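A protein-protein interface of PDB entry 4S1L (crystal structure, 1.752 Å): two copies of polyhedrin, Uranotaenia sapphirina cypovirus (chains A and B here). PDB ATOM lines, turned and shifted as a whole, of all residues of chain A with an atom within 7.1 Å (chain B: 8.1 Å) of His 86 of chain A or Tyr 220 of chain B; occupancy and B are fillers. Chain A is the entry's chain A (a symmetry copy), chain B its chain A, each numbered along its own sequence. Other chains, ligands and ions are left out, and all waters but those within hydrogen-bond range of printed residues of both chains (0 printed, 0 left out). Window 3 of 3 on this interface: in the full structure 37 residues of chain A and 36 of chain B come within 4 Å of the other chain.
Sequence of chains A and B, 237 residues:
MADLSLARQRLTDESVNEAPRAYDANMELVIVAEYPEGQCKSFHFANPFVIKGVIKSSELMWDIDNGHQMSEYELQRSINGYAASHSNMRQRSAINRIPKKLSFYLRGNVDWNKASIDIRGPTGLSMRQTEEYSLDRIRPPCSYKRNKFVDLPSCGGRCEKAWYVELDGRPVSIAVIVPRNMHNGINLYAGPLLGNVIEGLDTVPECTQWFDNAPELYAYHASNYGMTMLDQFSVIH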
ATOM      1  N   ASN A  80     -15.674  -3.624  16.418  1.00  0.00           N
ATOM      2  CA  ASN A  80     -14.650  -3.612  17.464  1.00  0.00           C
ATOM      3  C   ASN A  80     -15.216  -3.809  18.874  1.00  0.00           C
ATOM      4  O   ASN A  80     -14.626  -4.508  19.690  1.00  0.00           O
ATOM      5  CB  ASN A  80     -13.853  -2.295  17.433  1.00  0.00           C
ATOM      6  CG  ASN A  80     -12.800  -2.256  16.332  1.00  0.00           C
ATOM      7  OD1 ASN A  80     -12.411  -3.278  15.767  1.00  0.00           O
ATOM      8  ND2 ASN A  80     -12.335  -1.056  16.024  1.00  0.00           N
ATOM      9  N   GLY A  81     -16.366  -3.204  19.147  1.00  0.00           N
ATOM     10  CA  GLY A  81     -16.961  -3.267  20.470  1.00  0.00           C
ATOM     11  C   GLY A  81     -17.403  -4.669  20.887  1.00  0.00           C
ATOM     12  O   GLY A  81     -17.580  -4.964  22.069  1.00  0.00           O
ATOM     13  N   TYR A  82     -17.612  -5.538  19.912  1.00  0.00           N
ATOM     14  CA  TYR A  82     -17.886  -6.936  20.208  1.00  0.00           C
ATOM     15  C   TYR A  82     -16.604  -7.737  20.458  1.00  0.00           C
ATOM     16  O   TYR A  82     -16.638  -8.757  21.135  1.00  0.00           O
ATOM     17  CB  TYR A  82     -18.652  -7.580  19.056  1.00  0.00           C
ATOM     18  CG  TYR A  82     -20.041  -7.023  18.833  1.00  0.00           C
ATOM     19  CD1 TYR A  82     -20.250  -5.944  17.995  1.00  0.00           C
ATOM     20  CD2 TYR A  82     -21.149  -7.606  19.444  1.00  0.00           C
ATOM     21  CE1 TYR A  82     -21.526  -5.445  17.774  1.00  0.00           C
ATOM     22  CE2 TYR A  82     -22.424  -7.116  19.226  1.00  0.00           C
ATOM     23  CZ  TYR A  82     -22.609  -6.044  18.395  1.00  0.00           C
ATOM     24  OH  TYR A  82     -23.897  -5.566  18.183  1.00  0.00           O
ATOM     25  N   ALA A  83     -15.499  -7.283  19.877  1.00  0.00           N
ATOM     26  CA  ALA A  83     -14.225  -7.990  19.980  1.00  0.00           C
ATOM     27  C   ALA A  83     -13.488  -7.630  21.253  1.00  0.00           C
ATOM     28  O   ALA A  83     -12.896  -8.496  21.900  1.00  0.00           O
ATOM     29  CB  ALA A  83     -13.350  -7.670  18.781  1.00  0.00           C
ATOM     30  N   ALA A  84     -13.492  -6.334  21.576  1.00  0.00           N
ATOM     31  CA  ALA A  84     -12.791  -5.812  22.746  1.00  0.00           C
ATOM     32  C   ALA A  84     -13.723  -4.888  23.513  1.00  0.00           C
ATOM     33  O   ALA A  84     -14.269  -3.958  22.935  1.00  0.00           O
ATOM     34  CB  ALA A  84     -11.548  -5.070  22.338  1.00  0.00           C
ATOM     35  N   SER A  85     -13.959  -5.194  24.787  1.00  0.00           N
ATOM     36  CA  SER A  85     -14.838  -4.383  25.621  1.00  0.00           C
ATOM     37  C   SER A  85     -14.476  -2.897  25.598  1.00  0.00           C
ATOM     38  O   SER A  85     -13.328  -2.538  25.757  1.00  0.00           O
ATOM     39  CB  SER A  85     -14.797  -4.889  27.066  1.00  0.00           C
ATOM     40  OG  SER A  85     -15.332  -6.196  27.129  1.00  0.00           O
ATOM     41  N   HIS A  86     -15.496  -2.061  25.407  1.00  0.00           N
ATOM     42  CA  HIS A  86     -15.405  -0.598  25.421  1.00  0.00           C
ATOM     43  C   HIS A  86     -14.247  -0.043  24.572  1.00  0.00           C
ATOM     44  O   HIS A  86     -13.489   0.854  24.982  1.00  0.00           O
ATOM     45  CB  HIS A  86     -15.390  -0.052  26.873  1.00  0.00           C
ATOM     46  CG  HIS A  86     -14.266  -0.519  27.760  1.00  0.00           C
ATOM     47  ND1 HIS A  86     -12.974  -0.054  27.641  1.00  0.00           N
ATOM     48  CD2 HIS A  86     -14.274  -1.315  28.861  1.00  0.00           C
ATOM     49  CE1 HIS A  86     -12.223  -0.581  28.596  1.00  0.00           C
ATOM     50  NE2 HIS A  86     -12.986  -1.353  29.352  1.00  0.00           N
ATOM     51  N   SER A  87     -14.190  -0.531  23.333  1.00  0.00           N
ATOM     52  CA  SER A  87     -13.185  -0.113  22.375  1.00  0.00           C
ATOM     53  C   SER A  87     -13.743   0.833  21.282  1.00  0.00           C
ATOM     54  O   SER A  87     -12.992   1.321  20.423  1.00  0.00           O
ATOM     55  CB  SER A  87     -12.547  -1.347  21.740  1.00  0.00           C
ATOM     56  OG  SER A  87     -13.457  -2.058  20.921  1.00  0.00           O
ATOM     57  N   ASN A  88     -15.055   1.074  21.308  1.00  0.00           N
ATOM     58  CA  ASN A  88     -15.647   2.127  20.481  1.00  0.00           C
ATOM     59  C   ASN A  88     -16.552   2.961  21.364  1.00  0.00           C
ATOM     60  O   ASN A  88     -16.550   2.772  22.593  1.00  0.00           O
ATOM     61  CB  ASN A  88     -16.389   1.533  19.273  1.00  0.00           C
ATOM     62  CG  ASN A  88     -17.614   0.690  19.655  1.00  0.00           C
ATOM     63  OD1 ASN A  88     -18.198   0.852  20.720  1.00  0.00           O
ATOM     64  ND2 ASN A  88     -18.008  -0.211  18.757  1.00  0.00           N
ATOM     65  N   MET A  89     -17.320   3.869  20.758  1.00  0.00           N
ATOM     66  CA  MET A  89     -18.191   4.763  21.540  1.00  0.00           C
ATOM     67  C   MET A  89     -19.682   4.439  21.385  1.00  0.00           C
ATOM     68  O   MET A  89     -20.542   5.290  21.624  1.00  0.00           O
ATOM     69  CB  MET A  89     -17.921   6.219  21.148  1.00  0.00           C
ATOM     70  CG  MET A  89     -16.456   6.639  21.376  1.00  0.00           C
ATOM     71  SD  MET A  89     -16.011   6.551  23.119  1.00  0.00           S
ATOM     72  CE  MET A  89     -16.846   7.990  23.808  1.00  0.00           C
ATOM     73  N   GLN B 209      -7.519  -2.697  11.278  1.00  0.00           N
ATOM     74  CA  GLN B 209      -8.084  -1.868  12.331  1.00  0.00           C
ATOM     75  C   GLN B 209      -7.377  -0.522  12.351  1.00  0.00           C
ATOM     76  O   GLN B 209      -6.213  -0.416  11.977  1.00  0.00           O
ATOM     77  CB  GLN B 209      -7.989  -2.573  13.680  1.00  0.00           C
ATOM     78  CG  GLN B 209      -9.013  -3.699  13.907  1.00  0.00           C
ATOM     79  CD  GLN B 209      -8.736  -4.458  15.177  1.00  0.00           C
ATOM     80  OE1 GLN B 209      -7.641  -4.951  15.365  1.00  0.00           O
ATOM     81  NE2 GLN B 209      -9.706  -4.517  16.075  1.00  0.00           N
ATOM     82  N   PHE B 211      -6.627   2.970  14.839  1.00  0.00           N
ATOM     83  CA  PHE B 211      -6.551   3.480  16.217  1.00  0.00           C
ATOM     84  C   PHE B 211      -6.034   4.909  16.189  1.00  0.00           C
ATOM     85  O   PHE B 211      -5.160   5.229  15.384  1.00  0.00           O
ATOM     86  CB  PHE B 211      -5.638   2.581  17.074  1.00  0.00           C
ATOM     87  CG  PHE B 211      -6.061   1.139  17.090  1.00  0.00           C
ATOM     88  CD1 PHE B 211      -6.998   0.694  17.993  1.00  0.00           C
ATOM     89  CD2 PHE B 211      -5.528   0.228  16.185  1.00  0.00           C
ATOM     90  CE1 PHE B 211      -7.412  -0.635  18.006  1.00  0.00           C
ATOM     91  CE2 PHE B 211      -5.942  -1.113  16.204  1.00  0.00           C
ATOM     92  CZ  PHE B 211      -6.871  -1.530  17.128  1.00  0.00           C
ATOM     93  N   ASN B 213      -4.451   6.387  18.621  1.00  0.00           N
ATOM     94  CA  ASN B 213      -3.156   6.423  19.305  1.00  0.00           C
ATOM     95  C   ASN B 213      -2.698   5.024  19.740  1.00  0.00           C
ATOM     96  O   ASN B 213      -3.478   4.051  19.738  1.00  0.00           O
ATOM     97  CB  ASN B 213      -3.194   7.378  20.517  1.00  0.00           C
ATOM     98  CG  ASN B 213      -4.275   7.013  21.541  1.00  0.00           C
ATOM     99  OD1 ASN B 213      -4.326   5.886  22.052  1.00  0.00           O
ATOM    100  ND2 ASN B 213      -5.126   7.988  21.873  1.00  0.00           N
ATOM    101  N   ALA B 214      -1.424   4.910  20.097  1.00  0.00           N
ATOM    102  CA  ALA B 214      -0.843   3.593  20.403  1.00  0.00           C
ATOM    103  C   ALA B 214      -1.475   2.942  21.629  1.00  0.00           C
ATOM    104  O   ALA B 214      -1.678   1.722  21.655  1.00  0.00           O
ATOM    105  CB  ALA B 214       0.672   3.704  20.607  1.00  0.00           C
ATOM    106  N   PRO B 215      -1.734   3.737  22.683  1.00  0.00           N
ATOM    107  CA  PRO B 215      -2.370   3.104  23.849  1.00  0.00           C
ATOM    108  C   PRO B 215      -3.711   2.376  23.518  1.00  0.00           C
ATOM    109  O   PRO B 215      -3.961   1.307  24.083  1.00  0.00           O
ATOM    110  CB  PRO B 215      -2.582   4.279  24.811  1.00  0.00           C
ATOM    111  CG  PRO B 215      -1.451   5.223  24.490  1.00  0.00           C
ATOM    112  CD  PRO B 215      -1.243   5.097  22.984  1.00  0.00           C
ATOM    113  N   GLU B 216      -4.549   2.930  22.634  1.00  0.00           N
ATOM    114  CA  GLU B 216      -5.734   2.211  22.161  1.00  0.00           C
ATOM    115  C   GLU B 216      -5.377   0.871  21.526  1.00  0.00           C
ATOM    116  O   GLU B 216      -6.065  -0.131  21.760  1.00  0.00           O
ATOM    117  CB  GLU B 216      -6.526   3.043  21.125  1.00  0.00           C
ATOM    118  CG  GLU B 216      -7.192   4.268  21.683  1.00  0.00           C
ATOM    119  CD  GLU B 216      -7.840   5.152  20.616  1.00  0.00           C
ATOM    120  OE1 GLU B 216      -7.755   4.834  19.413  1.00  0.00           O
ATOM    121  OE2 GLU B 216      -8.413   6.188  21.005  1.00  0.00           O
ATOM    122  N   LEU B 217      -4.348   0.876  20.672  1.00  0.00           N
ATOM    123  CA  LEU B 217      -3.829  -0.353  20.062  1.00  0.00           C
ATOM    124  C   LEU B 217      -3.410  -1.366  21.147  1.00  0.00           C
ATOM    125  O   LEU B 217      -3.747  -2.569  21.082  1.00  0.00           O
ATOM    126  CB  LEU B 217      -2.632  -0.026  19.142  1.00  0.00           C
ATOM    127  CG  LEU B 217      -1.850  -1.201  18.528  1.00  0.00           C
ATOM    128  CD1 LEU B 217      -2.683  -1.846  17.433  1.00  0.00           C
ATOM    129  CD2 LEU B 217      -0.513  -0.712  18.017  1.00  0.00           C
ATOM    130  N   TYR B 218      -2.681  -0.883  22.152  1.00  0.00           N
ATOM    131  CA  TYR B 218      -2.231  -1.766  23.235  1.00  0.00           C
ATOM    132  C   TYR B 218      -3.417  -2.334  24.026  1.00  0.00           C
ATOM    133  O   TYR B 218      -3.463  -3.527  24.326  1.00  0.00           O
ATOM    134  CB  TYR B 218      -1.279  -1.042  24.211  1.00  0.00           C
ATOM    135  CG  TYR B 218      -0.072  -0.404  23.566  1.00  0.00           C
ATOM    136  CD1 TYR B 218       0.481  -0.927  22.413  1.00  0.00           C
ATOM    137  CD2 TYR B 218       0.512   0.741  24.116  1.00  0.00           C
ATOM    138  CE1 TYR B 218       1.583  -0.327  21.811  1.00  0.00           C
ATOM    139  CE2 TYR B 218       1.596   1.346  23.522  1.00  0.00           C
ATOM    140  CZ  TYR B 218       2.137   0.802  22.368  1.00  0.00           C
ATOM    141  OH  TYR B 218       3.227   1.372  21.742  1.00  0.00           O
ATOM    142  N   ALA B 219      -4.372  -1.479  24.367  1.00  0.00           N
ATOM    143  CA  ALA B 219      -5.490  -1.871  25.212  1.00  0.00           C
ATOM    144  C   ALA B 219      -6.492  -2.778  24.508  1.00  0.00           C
ATOM    145  O   ALA B 219      -7.038  -3.709  25.105  1.00  0.00           O
ATOM    146  CB  ALA B 219      -6.197  -0.615  25.734  1.00  0.00           C
ATOM    147  N   TYR B 220      -6.742  -2.524  23.241  1.00  0.00           N
ATOM    148  CA  TYR B 220      -7.879  -3.168  22.573  1.00  0.00           C
ATOM    149  C   TYR B 220      -7.480  -4.136  21.461  1.00  0.00           C
ATOM    150  O   TYR B 220      -8.356  -4.761  20.872  1.00  0.00           O
ATOM    151  CB  TYR B 220      -8.820  -2.094  22.030  1.00  0.00           C
ATOM    152  CG  TYR B 220      -9.316  -1.204  23.150  1.00  0.00           C
ATOM    153  CD1 TYR B 220      -9.757  -1.767  24.336  1.00  0.00           C
ATOM    154  CD2 TYR B 220      -9.287   0.186  23.051  1.00  0.00           C
ATOM    155  CE1 TYR B 220     -10.193  -0.980  25.401  1.00  0.00           C
ATOM    156  CE2 TYR B 220      -9.715   0.990  24.121  1.00  0.00           C
ATOM    157  CZ  TYR B 220     -10.167   0.391  25.293  1.00  0.00           C
ATOM    158  OH  TYR B 220     -10.600   1.126  26.360  1.00  0.00           O
ATOM    159  N   HIS B 221      -6.179  -4.268  21.190  1.00  0.00           N
ATOM    160  CA  HIS B 221      -5.670  -5.304  20.285  1.00  0.00           C
ATOM    161  C   HIS B 221      -4.629  -6.161  21.012  1.00  0.00           C
ATOM    162  O   HIS B 221      -4.893  -7.330  21.320  1.00  0.00           O
ATOM    163  CB  HIS B 221      -5.074  -4.662  18.998  1.00  0.00           C
ATOM    164  CG  HIS B 221      -4.697  -5.643  17.928  1.00  0.00           C
ATOM    165  ND1 HIS B 221      -4.023  -6.817  18.190  1.00  0.00           N
ATOM    166  CD2 HIS B 221      -4.863  -5.600  16.584  1.00  0.00           C
ATOM    167  CE1 HIS B 221      -3.815  -7.467  17.057  1.00  0.00           C
ATOM    168  NE2 HIS B 221      -4.311  -6.749  16.068  1.00  0.00           N
ATOM    169  N   ALA B 222      -3.456  -5.584  21.277  1.00  0.00           N
ATOM    170  CA  ALA B 222      -2.308  -6.348  21.805  1.00  0.00           C
ATOM    171  C   ALA B 222      -2.659  -7.162  23.055  1.00  0.00           C
ATOM    172  O   ALA B 222      -2.465  -8.389  23.095  1.00  0.00           O
ATOM    173  CB  ALA B 222      -1.141  -5.400  22.109  1.00  0.00           C
ATOM    174  N   SER B 223      -3.195  -6.481  24.068  1.00  0.00           N
ATOM    175  CA  SER B 223      -3.473  -7.140  25.345  1.00  0.00           C
ATOM    176  C   SER B 223      -4.813  -7.861  25.326  1.00  0.00           C
ATOM    177  O   SER B 223      -5.098  -8.639  26.217  1.00  0.00           O
ATOM    178  CB  SER B 223      -3.450  -6.132  26.514  1.00  0.00           C
ATOM    179  OG  SER B 223      -4.527  -5.196  26.452  1.00  0.00           O
ATOM    180  N   ASN B 224      -5.624  -7.616  24.303  1.00  0.00           N
ATOM    181  CA  ASN B 224      -6.885  -8.341  24.185  1.00  0.00           C
ATOM    182  C   ASN B 224      -6.624  -9.766  23.717  1.00  0.00           C
ATOM    183  O   ASN B 224      -7.271 -10.709  24.181  1.00  0.00           O
ATOM    184  CB  ASN B 224      -7.824  -7.632  23.209  1.00  0.00           C
ATOM    185  CG  ASN B 224      -9.289  -8.034  23.394  1.00  0.00           C
ATOM    186  OD1 ASN B 224      -9.837  -7.933  24.489  1.00  0.00           O
ATOM    187  ND2 ASN B 224      -9.923  -8.486  22.317  1.00  0.00           N
ATOM    188  N   TYR B 225      -5.637  -9.923  22.825  1.00  0.00           N
ATOM    189  CA  TYR B 225      -5.423 -11.205  22.136  1.00  0.00           C
ATOM    190  C   TYR B 225      -4.093 -11.882  22.406  1.00  0.00           C
ATOM    191  O   TYR B 225      -3.870 -13.000  21.975  1.00  0.00           O
ATOM    192  CB  TYR B 225      -5.550 -11.014  20.629  1.00  0.00           C
ATOM    193  CG  TYR B 225      -6.940 -10.677  20.148  1.00  0.00           C
ATOM    194  CD1 TYR B 225      -8.049 -11.419  20.552  1.00  0.00           C
ATOM    195  CD2 TYR B 225      -7.148  -9.612  19.278  1.00  0.00           C
ATOM    196  CE1 TYR B 225      -9.309 -11.106  20.090  1.00  0.00           C
ATOM    197  CE2 TYR B 225      -8.408  -9.309  18.809  1.00  0.00           C
ATOM    198  CZ  TYR B 225      -9.482 -10.056  19.219  1.00  0.00           C
ATOM    199  OH  TYR B 225     -10.732  -9.728  18.739  1.00  0.00           O
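The backbone carbonyl oxygen (O) of Asn 80 of chain A sits at hydrogen-bond distance from the side-chain hydroxyl (OG) of Ser 87 of chain A (3.0 Å). The side-chain hydroxyl of Ser 87 of chain A lies within hydrogen-bond range of the backbone carbonyl oxygen of Ala 84 of chain A.
Tyr 220 of chain B touches four residues of chain A. Of the printed residues of chain B, Asn 80 of chain A touches Gln 209 (3.0 Å). Of the printed residues of chain B, Ser 85 of chain A touches Tyr 220 (3.5 Å). Of the printed residues of chain A, Tyr 225 of chain B touches Ala 83 (3.3 Å). Tyr 82 of chain A touches none of the printed residues of chain B. The nearest printed residue of chain B that does not touch Ser 85 of chain A is Asn 224 of chain B (5.0 Å).
No position is printed for both chains. Of the 8 pairs that touch across the chains among the printed residues, none has its exchanged pair printed and touching as well.
Ala 83 of chain A touches Tyr 225 of chain B (CB to OH, 3.3 Å). CB of Ala 84 of chain A touches O of Tyr 220 of chain B (3.5 Å). Ala 84 of chain A touches Asn 224 of chain B. Ser 85 of chain A touches Tyr 220 of chain B. CB of Ser 87 of chain A touches CG of Tyr 220 of chain B, 3.5 Å away.
Printed residues of chain A that touch a printed residue of chain B: Asn 80, Ala 83, Ala 84, Ser 85, His 86 and Ser 87. Hydrophobic or aromatic side chains of chain A within 4 Å of the printed part of chain B: Ala 83, Ala 84 and His 86. Of the 15 printed residues of chain B, 4 touch a printed residue of chain A. Hydrophobic or aromatic side chains of chain B within 4 Å of the printed part of chain A: Tyr 220 and Tyr 225. Among the printed residues, 8 pairs touch across the chains.
The side-chain amide oxygen (OD1) of Asn 80 of chain A lies within hydrogen-bond range of the side-chain amide nitrogen (NE2) of Gln 209 of chain B (3.0 Å). OH of Tyr 220 of chain B lies within hydrogen-bond range of ND1 of His 86 of chain A, at 2.9 Å. The backbone carbonyl oxygen of Ala 83 of chain A is in hydrogen-bond range of the side-chain amide nitrogen of Asn 224 of chain B (3.0 Å).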
